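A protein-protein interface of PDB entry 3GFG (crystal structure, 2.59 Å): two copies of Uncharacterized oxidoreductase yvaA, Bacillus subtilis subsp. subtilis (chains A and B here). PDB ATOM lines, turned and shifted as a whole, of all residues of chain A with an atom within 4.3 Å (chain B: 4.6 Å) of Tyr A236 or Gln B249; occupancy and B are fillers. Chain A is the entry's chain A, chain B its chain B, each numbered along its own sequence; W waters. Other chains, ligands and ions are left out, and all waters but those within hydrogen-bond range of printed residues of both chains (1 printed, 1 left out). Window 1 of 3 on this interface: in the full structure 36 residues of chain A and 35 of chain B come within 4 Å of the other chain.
The side-chain hydroxyl (OH) of Tyr A236 lies within hydrogen-bond range of the side-chain amide oxygen (OE1) of Gln B159, 3.2 Å away.
The backbone NH (N) of Tyr A236 lies within hydrogen-bond range of the backbone carbonyl oxygen (O) of Val A160 (3.0 Å). The backbone carbonyl oxygen of Pro A246 is in hydrogen-bond range of the side-chain hydroxyl of Ser A161, at 3.0 Å. The backbone carbonyl oxygen (O) of Tyr A236 sits at hydrogen-bond distance from the backbone NH (N) of Tyr A162 (2.8 Å). The backbone NH of Gln B159 lies within hydrogen-bond range of the backbone carbonyl oxygen of Gln B249, 2.8 Å away.
Among the printed residues, pairs that only touch across the chains: Tyr A236 with Gln B249 (3.9 Å), Asn A244 with Gln B249 (3.6 Å), Gly A245 with Gln B249 (3.5 Å), Pro A246 with Pro B246 (3.7 Å) and Gln A249 with Pro B246 (3.7 Å).
Of chain B, only Gln B159 and Gln B249 come within 4 Å of Tyr A236. Printed residues of chain A within 4 Å of Gln B249: Tyr A236 (3.9 Å), Asn A244 (3.6 Å) and Gly A245 (3.5 Å). Of the printed residues of chain B, Gln A249 touches Pro B246. Of the printed residues of chain B, Gly A245 touches Gln B249 (3.5 Å). Printed residues of chain B within 4 Å of Pro A246: Pro B246. Of the printed residues of chain A, Pro B246 touches Pro A246 (3.7 Å) and Gln A249 (3.7 Å). His A223 touches none of the printed residues of chain B. The nearest printed residue of chain B that does not touch Tyr A236 is Thr B157 (6.2 Å). The nearest printed residue of chain B that does not touch Pro A246 is Gln B249 (4.001 Å).
Hydrophobic or aromatic side chains of chain A within 4 Å of the printed part of chain B: Tyr A236 and Pro A246. Hydrophobic or aromatic side chains of chain B that line the printed part of chain A: Pro B246. Among the printed residues, no Asp or Glu carboxylate lies within 4 Å of a Lys or Arg side-chain nitrogen of the other chain.
Pro A246 touches its own counterpart, Pro B246. Gln A249 touches Pro B246, but with the chains exchanged Pro A246 does not touch Gln B249 (4.001 Å).
Water W1 lies within hydrogen-bond range of the backbone carbonyl oxygen (O) of Pro B246 (2.6 Å) and the side-chain amide nitrogen (NE2) of Gln A249 (3.1 Å).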
ATOM      1  N   VAL A 160       4.602 -14.451 -14.056  1.00  0.00           N
ATOM      2  CA  VAL A 160       6.029 -14.259 -13.985  1.00  0.00           C
ATOM      3  C   VAL A 160       6.371 -13.582 -12.693  1.00  0.00           C
ATOM      4  O   VAL A 160       5.792 -12.551 -12.353  1.00  0.00           O
ATOM      5  CB  VAL A 160       6.549 -13.430 -15.193  1.00  0.00           C
ATOM      6  CG1 VAL A 160       8.087 -13.330 -15.175  1.00  0.00           C
ATOM      7  CG2 VAL A 160       6.046 -14.051 -16.523  1.00  0.00           C
ATOM      8  N   SER A 161       7.288 -14.170 -11.937  1.00  0.00           N
ATOM      9  CA  SER A 161       7.711 -13.516 -10.712  1.00  0.00           C
ATOM     10  C   SER A 161       9.186 -13.130 -10.739  1.00  0.00           C
ATOM     11  O   SER A 161      10.000 -13.878 -11.215  1.00  0.00           O
ATOM     12  CB  SER A 161       7.387 -14.367  -9.502  1.00  0.00           C
ATOM     13  OG  SER A 161       8.296 -15.411  -9.465  1.00  0.00           O
ATOM     14  N   TYR A 162       9.510 -11.955 -10.221  1.00  0.00           N
ATOM     15  CA  TYR A 162      10.880 -11.469 -10.196  1.00  0.00           C
ATOM     16  C   TYR A 162      11.162 -10.976  -8.769  1.00  0.00           C
ATOM     17  O   TYR A 162      11.115  -9.782  -8.479  1.00  0.00           O
ATOM     18  CB  TYR A 162      11.016 -10.341 -11.216  1.00  0.00           C
ATOM     19  CG  TYR A 162      12.418  -9.996 -11.670  1.00  0.00           C
ATOM     20  CD1 TYR A 162      12.632  -9.387 -12.911  1.00  0.00           C
ATOM     21  CD2 TYR A 162      13.522 -10.269 -10.871  1.00  0.00           C
ATOM     22  CE1 TYR A 162      13.910  -9.048 -13.335  1.00  0.00           C
ATOM     23  CE2 TYR A 162      14.801  -9.930 -11.279  1.00  0.00           C
ATOM     24  CZ  TYR A 162      14.994  -9.320 -12.511  1.00  0.00           C
ATOM     25  OH  TYR A 162      16.278  -8.998 -12.899  1.00  0.00           O
ATOM     26  N   PHE A 222       5.646  -4.992  -6.431  1.00  0.00           N
ATOM     27  CA  PHE A 222       4.658  -4.712  -7.460  1.00  0.00           C
ATOM     28  C   PHE A 222       3.908  -5.962  -7.836  1.00  0.00           C
ATOM     29  O   PHE A 222       4.469  -7.071  -7.865  1.00  0.00           O
ATOM     30  CB  PHE A 222       5.289  -4.083  -8.702  1.00  0.00           C
ATOM     31  CG  PHE A 222       6.285  -4.957  -9.388  1.00  0.00           C
ATOM     32  CD1 PHE A 222       5.891  -5.834 -10.390  1.00  0.00           C
ATOM     33  CD2 PHE A 222       7.613  -4.903  -9.033  1.00  0.00           C
ATOM     34  CE1 PHE A 222       6.820  -6.668 -11.025  1.00  0.00           C
ATOM     35  CE2 PHE A 222       8.558  -5.713  -9.658  1.00  0.00           C
ATOM     36  CZ  PHE A 222       8.167  -6.599 -10.653  1.00  0.00           C
ATOM     37  N   HIS A 223       2.625  -5.775  -8.118  1.00  0.00           N
ATOM     38  CA  HIS A 223       1.792  -6.855  -8.618  1.00  0.00           C
ATOM     39  C   HIS A 223       0.846  -6.344  -9.709  1.00  0.00           C
ATOM     40  O   HIS A 223      -0.146  -5.682  -9.432  1.00  0.00           O
ATOM     41  CB  HIS A 223       1.038  -7.546  -7.488  1.00  0.00           C
ATOM     42  CG  HIS A 223       0.339  -8.783  -7.927  1.00  0.00           C
ATOM     43  ND1 HIS A 223      -0.817  -8.748  -8.680  1.00  0.00           N
ATOM     44  CD2 HIS A 223       0.642 -10.093  -7.752  1.00  0.00           C
ATOM     45  CE1 HIS A 223      -1.200  -9.988  -8.944  1.00  0.00           C
ATOM     46  NE2 HIS A 223      -0.330 -10.822  -8.395  1.00  0.00           N
ATOM     47  N   ILE A 234       0.246 -12.109 -15.352  1.00  0.00           N
ATOM     48  CA  ILE A 234       0.475 -11.631 -13.992  1.00  0.00           C
ATOM     49  C   ILE A 234       1.959 -11.419 -13.816  1.00  0.00           C
ATOM     50  O   ILE A 234       2.745 -12.353 -13.965  1.00  0.00           O
ATOM     51  CB  ILE A 234       0.023 -12.661 -12.913  1.00  0.00           C
ATOM     52  CG1 ILE A 234      -1.288 -13.324 -13.296  1.00  0.00           C
ATOM     53  CG2 ILE A 234      -0.080 -12.007 -11.545  1.00  0.00           C
ATOM     54  CD1 ILE A 234      -2.458 -12.512 -13.029  1.00  0.00           C
ATOM     55  N   LEU A 235       2.345 -10.198 -13.507  1.00  0.00           N
ATOM     56  CA  LEU A 235       3.750  -9.856 -13.330  1.00  0.00           C
ATOM     57  C   LEU A 235       3.913  -9.316 -11.914  1.00  0.00           C
ATOM     58  O   LEU A 235       3.253  -8.313 -11.518  1.00  0.00           O
ATOM     59  CB  LEU A 235       4.143  -8.809 -14.371  1.00  0.00           C
ATOM     60  CG  LEU A 235       3.733  -9.166 -15.810  1.00  0.00           C
ATOM     61  CD1 LEU A 235       4.072  -8.057 -16.732  1.00  0.00           C
ATOM     62  CD2 LEU A 235       4.397 -10.489 -16.296  1.00  0.00           C
ATOM     63  N   TYR A 236       4.739 -10.003 -11.123  1.00  0.00           N
ATOM     64  CA  TYR A 236       4.945  -9.577  -9.744  1.00  0.00           C
ATOM     65  C   TYR A 236       6.315  -9.841  -9.201  1.00  0.00           C
ATOM     66  O   TYR A 236       7.078 -10.684  -9.720  1.00  0.00           O
ATOM     67  CB  TYR A 236       3.905 -10.177  -8.805  1.00  0.00           C
ATOM     68  CG  TYR A 236       4.024 -11.658  -8.612  1.00  0.00           C
ATOM     69  CD1 TYR A 236       4.754 -12.184  -7.545  1.00  0.00           C
ATOM     70  CD2 TYR A 236       3.406 -12.549  -9.521  1.00  0.00           C
ATOM     71  CE1 TYR A 236       4.854 -13.552  -7.357  1.00  0.00           C
ATOM     72  CE2 TYR A 236       3.510 -13.935  -9.365  1.00  0.00           C
ATOM     73  CZ  TYR A 236       4.224 -14.438  -8.266  1.00  0.00           C
ATOM     74  OH  TYR A 236       4.331 -15.816  -8.098  1.00  0.00           O
ATOM     75  N   GLY A 237       6.615  -9.104  -8.132  1.00  0.00           N
ATOM     76  CA  GLY A 237       7.878  -9.237  -7.448  1.00  0.00           C
ATOM     77  C   GLY A 237       7.791  -8.562  -6.116  1.00  0.00           C
ATOM     78  O   GLY A 237       7.102  -7.549  -5.984  1.00  0.00           O
ATOM     79  N   ASN A 244      12.179 -18.142  -4.003  1.00  0.00           N
ATOM     80  CA  ASN A 244      11.433 -17.577  -5.104  1.00  0.00           C
ATOM     81  C   ASN A 244      10.140 -18.212  -5.527  1.00  0.00           C
ATOM     82  O   ASN A 244       9.173 -17.479  -5.872  1.00  0.00           O
ATOM     83  CB  ASN A 244      12.315 -17.534  -6.345  1.00  0.00           C
ATOM     84  CG  ASN A 244      13.358 -16.500  -6.247  1.00  0.00           C
ATOM     85  OD1 ASN A 244      13.168 -15.496  -5.568  1.00  0.00           O
ATOM     86  ND2 ASN A 244      14.490 -16.725  -6.905  1.00  0.00           N
ATOM     87  N   GLY A 245      10.106 -19.540  -5.615  1.00  0.00           N
ATOM     88  CA  GLY A 245       9.009 -20.125  -6.395  1.00  0.00           C
ATOM     89  C   GLY A 245       9.318 -19.948  -7.883  1.00  0.00           C
ATOM     90  O   GLY A 245      10.261 -19.212  -8.249  1.00  0.00           O
ATOM     91  N   PRO A 246       8.543 -20.603  -8.759  1.00  0.00           N
ATOM     92  CA  PRO A 246       8.864 -20.557 -10.185  1.00  0.00           C
ATOM     93  C   PRO A 246       8.910 -19.126 -10.726  1.00  0.00           C
ATOM     94  O   PRO A 246       8.134 -18.285 -10.292  1.00  0.00           O
ATOM     95  CB  PRO A 246       7.698 -21.301 -10.844  1.00  0.00           C
ATOM     96  CG  PRO A 246       6.716 -21.575  -9.823  1.00  0.00           C
ATOM     97  CD  PRO A 246       7.170 -21.070  -8.510  1.00  0.00           C
ATOM     98  N   GLN A 249       5.177 -19.403 -14.870  1.00  0.00           N
ATOM     99  CA  GLN A 249       4.141 -20.406 -14.921  1.00  0.00           C
ATOM    100  C   GLN A 249       3.288 -20.022 -16.105  1.00  0.00           C
ATOM    101  O   GLN A 249       2.669 -18.959 -16.108  1.00  0.00           O
ATOM    102  CB  GLN A 249       3.282 -20.427 -13.644  1.00  0.00           C
ATOM    103  CG  GLN A 249       4.042 -20.813 -12.376  1.00  0.00           C
ATOM    104  CD  GLN A 249       3.137 -20.940 -11.154  1.00  0.00           C
ATOM    105  OE1 GLN A 249       3.432 -20.389 -10.093  1.00  0.00           O
ATOM    106  NE2 GLN A 249       2.028 -21.658 -11.302  1.00  0.00           N
ATOM    107  N   THR B 157       3.887 -11.962   2.378  1.00  0.00           N
ATOM    108  CA  THR B 157       3.214 -12.415   1.166  1.00  0.00           C
ATOM    109  C   THR B 157       2.686 -13.833   1.341  1.00  0.00           C
ATOM    110  O   THR B 157       3.397 -14.731   1.836  1.00  0.00           O
ATOM    111  CB  THR B 157       4.139 -12.323  -0.095  1.00  0.00           C
ATOM    112  OG1 THR B 157       4.688 -10.996  -0.206  1.00  0.00           O
ATOM    113  CG2 THR B 157       3.357 -12.669  -1.379  1.00  0.00           C
ATOM    114  N   TYR B 158       1.446 -14.030   0.927  1.00  0.00           N
ATOM    115  CA  TYR B 158       0.761 -15.281   1.114  1.00  0.00           C
ATOM    116  C   TYR B 158       0.002 -15.576  -0.187  1.00  0.00           C
ATOM    117  O   TYR B 158      -1.027 -14.943  -0.443  1.00  0.00           O
ATOM    118  CB  TYR B 158      -0.196 -15.161   2.315  1.00  0.00           C
ATOM    119  CG  TYR B 158      -0.947 -16.422   2.644  1.00  0.00           C
ATOM    120  CD1 TYR B 158      -0.320 -17.473   3.329  1.00  0.00           C
ATOM    121  CD2 TYR B 158      -2.287 -16.574   2.285  1.00  0.00           C
ATOM    122  CE1 TYR B 158      -1.012 -18.651   3.651  1.00  0.00           C
ATOM    123  CE2 TYR B 158      -2.997 -17.747   2.607  1.00  0.00           C
ATOM    124  CZ  TYR B 158      -2.341 -18.786   3.280  1.00  0.00           C
ATOM    125  OH  TYR B 158      -2.999 -19.965   3.588  1.00  0.00           O
ATOM    126  N   GLN B 159       0.518 -16.494  -1.018  1.00  0.00           N
ATOM    127  CA  GLN B 159      -0.108 -16.774  -2.318  1.00  0.00           C
ATOM    128  C   GLN B 159      -0.544 -18.202  -2.425  1.00  0.00           C
ATOM    129  O   GLN B 159       0.272 -19.128  -2.281  1.00  0.00           O
ATOM    130  CB  GLN B 159       0.829 -16.501  -3.485  1.00  0.00           C
ATOM    131  CG  GLN B 159       1.430 -15.148  -3.499  1.00  0.00           C
ATOM    132  CD  GLN B 159       2.272 -14.910  -4.750  1.00  0.00           C
ATOM    133  OE1 GLN B 159       2.951 -15.830  -5.254  1.00  0.00           O
ATOM    134  NE2 GLN B 159       2.243 -13.660  -5.258  1.00  0.00           N
ATOM    135  N   PRO B 246       3.178 -24.194  -7.378  1.00  0.00           N
ATOM    136  CA  PRO B 246       2.949 -24.388  -5.963  1.00  0.00           C
ATOM    137  C   PRO B 246       1.510 -24.078  -5.581  1.00  0.00           C
ATOM    138  O   PRO B 246       0.929 -23.112  -6.081  1.00  0.00           O
ATOM    139  CB  PRO B 246       3.859 -23.338  -5.331  1.00  0.00           C
ATOM    140  CG  PRO B 246       4.884 -23.079  -6.365  1.00  0.00           C
ATOM    141  CD  PRO B 246       4.117 -23.096  -7.612  1.00  0.00           C
ATOM    142  N   ARG B 247       0.946 -24.897  -4.698  1.00  0.00           N
ATOM    143  CA  ARG B 247      -0.285 -24.501  -4.034  1.00  0.00           C
ATOM    144  C   ARG B 247      -0.062 -23.318  -3.062  1.00  0.00           C
ATOM    145  O   ARG B 247      -0.871 -22.405  -3.030  1.00  0.00           O
ATOM    146  CB  ARG B 247      -0.947 -25.687  -3.337  1.00  0.00           C
ATOM    147  CG  ARG B 247      -2.309 -25.335  -2.786  1.00  0.00           C
ATOM    148  CD  ARG B 247      -3.020 -26.534  -2.248  1.00  0.00           C
ATOM    149  NE  ARG B 247      -4.108 -26.160  -1.341  1.00  0.00           N
ATOM    150  CZ  ARG B 247      -5.391 -26.133  -1.692  1.00  0.00           C
ATOM    151  NH1 ARG B 247      -5.741 -26.429  -2.928  1.00  0.00           N
ATOM    152  NH2 ARG B 247      -6.319 -25.800  -0.810  1.00  0.00           N
ATOM    153  N   TYR B 248       1.014 -23.338  -2.276  1.00  0.00           N
ATOM    154  CA  TYR B 248       1.297 -22.244  -1.322  1.00  0.00           C
ATOM    155  C   TYR B 248       2.655 -21.684  -1.610  1.00  0.00           C
ATOM    156  O   TYR B 248       3.589 -22.416  -1.860  1.00  0.00           O
ATOM    157  CB  TYR B 248       1.277 -22.694   0.171  1.00  0.00           C
ATOM    158  CG  TYR B 248      -0.070 -23.187   0.641  1.00  0.00           C
ATOM    159  CD1 TYR B 248      -1.024 -22.298   1.139  1.00  0.00           C
ATOM    160  CD2 TYR B 248      -0.414 -24.531   0.548  1.00  0.00           C
ATOM    161  CE1 TYR B 248      -2.273 -22.737   1.544  1.00  0.00           C
ATOM    162  CE2 TYR B 248      -1.668 -24.979   0.952  1.00  0.00           C
ATOM    163  CZ  TYR B 248      -2.585 -24.071   1.442  1.00  0.00           C
ATOM    164  OH  TYR B 248      -3.829 -24.495   1.836  1.00  0.00           O
ATOM    165  N   GLN B 249       2.748 -20.369  -1.580  1.00  0.00           N
ATOM    166  CA  GLN B 249       4.011 -19.671  -1.508  1.00  0.00           C
ATOM    167  C   GLN B 249       3.828 -18.669  -0.397  1.00  0.00           C
ATOM    168  O   GLN B 249       2.985 -17.759  -0.476  1.00  0.00           O
ATOM    169  CB  GLN B 249       4.326 -18.994  -2.840  1.00  0.00           C
ATOM    170  CG  GLN B 249       4.498 -19.980  -4.011  1.00  0.00           C
ATOM    171  CD  GLN B 249       4.795 -19.273  -5.308  1.00  0.00           C
ATOM    172  OE1 GLN B 249       5.880 -18.776  -5.497  1.00  0.00           O
ATOM    173  NE2 GLN B 249       3.816 -19.206  -6.200  1.00  0.00           N
ATOM    174  N   ILE B 250       4.569 -18.865   0.676  1.00  0.00           N
ATOM    175  CA  ILE B 250       4.436 -17.980   1.821  1.00  0.00           C
ATOM    176  C   ILE B 250       5.781 -17.349   2.138  1.00  0.00           C
ATOM    177  O   ILE B 250       6.730 -18.044   2.371  1.00  0.00           O
ATOM    178  CB  ILE B 250       3.860 -18.745   3.039  1.00  0.00           C
ATOM    179  CG1 ILE B 250       2.527 -19.404   2.645  1.00  0.00           C
ATOM    180  CG2 ILE B 250       3.693 -17.809   4.228  1.00  0.00           C
ATOM    181  CD1 ILE B 250       2.097 -20.538   3.540  1.00  0.00           C
ATOM    182  N   HIS B 251       5.851 -16.030   2.129  1.00  0.00           N
ATOM    183  CA  HIS B 251       7.098 -15.334   2.472  1.00  0.00           C
ATOM    184  C   HIS B 251       6.982 -14.516   3.745  1.00  0.00           C
ATOM    185  O   HIS B 251       6.039 -13.718   3.910  1.00  0.00           O
ATOM    186  CB  HIS B 251       7.589 -14.460   1.304  1.00  0.00           C
ATOM    187  CG  HIS B 251       7.566 -15.170  -0.007  1.00  0.00           C
ATOM    188  ND1 HIS B 251       8.248 -16.351  -0.222  1.00  0.00           N
ATOM    189  CD2 HIS B 251       6.888 -14.908  -1.148  1.00  0.00           C
ATOM    190  CE1 HIS B 251       7.993 -16.780  -1.444  1.00  0.00           C
ATOM    191  NE2 HIS B 251       7.178 -15.919  -2.029  1.00  0.00           N
ATOM    192  N   PHE B 257       8.011 -20.652   2.732  1.00  0.00           N
ATOM    193  CA  PHE B 257       7.477 -22.010   2.602  1.00  0.00           C
ATOM    194  C   PHE B 257       6.776 -22.133   1.241  1.00  0.00           C
ATOM    195  O   PHE B 257       5.900 -21.341   0.931  1.00  0.00           O
ATOM    196  CB  PHE B 257       6.521 -22.283   3.744  1.00  0.00           C
ATOM    197  CG  PHE B 257       6.107 -23.717   3.869  1.00  0.00           C
ATOM    198  CD1 PHE B 257       7.034 -24.702   4.233  1.00  0.00           C
ATOM    199  CD2 PHE B 257       4.778 -24.089   3.651  1.00  0.00           C
ATOM    200  CE1 PHE B 257       6.654 -26.025   4.356  1.00  0.00           C
ATOM    201  CE2 PHE B 257       4.399 -25.418   3.782  1.00  0.00           C
ATOM    202  CZ  PHE B 257       5.336 -26.382   4.142  1.00  0.00           C
ATOM    203  N   ILE B 258       7.218 -23.071   0.408  1.00  0.00           N
ATOM    204  CA  ILE B 258       6.653 -23.279  -0.927  1.00  0.00           C
ATOM    205  C   ILE B 258       6.209 -24.722  -0.926  1.00  0.00           C
ATOM    206  O   ILE B 258       7.003 -25.601  -0.617  1.00  0.00           O
ATOM    207  CB  ILE B 258       7.709 -23.135  -2.102  1.00  0.00           C
ATOM    208  CG1 ILE B 258       8.660 -21.929  -1.953  1.00  0.00           C
ATOM    209  CG2 ILE B 258       7.025 -23.155  -3.493  1.00  0.00           C
ATOM    210  CD1 ILE B 258       8.049 -20.613  -2.221  1.00  0.00           C
HETATM  211  O   HOH W   1       0.991 -21.897  -8.371  1.00  0.00           O
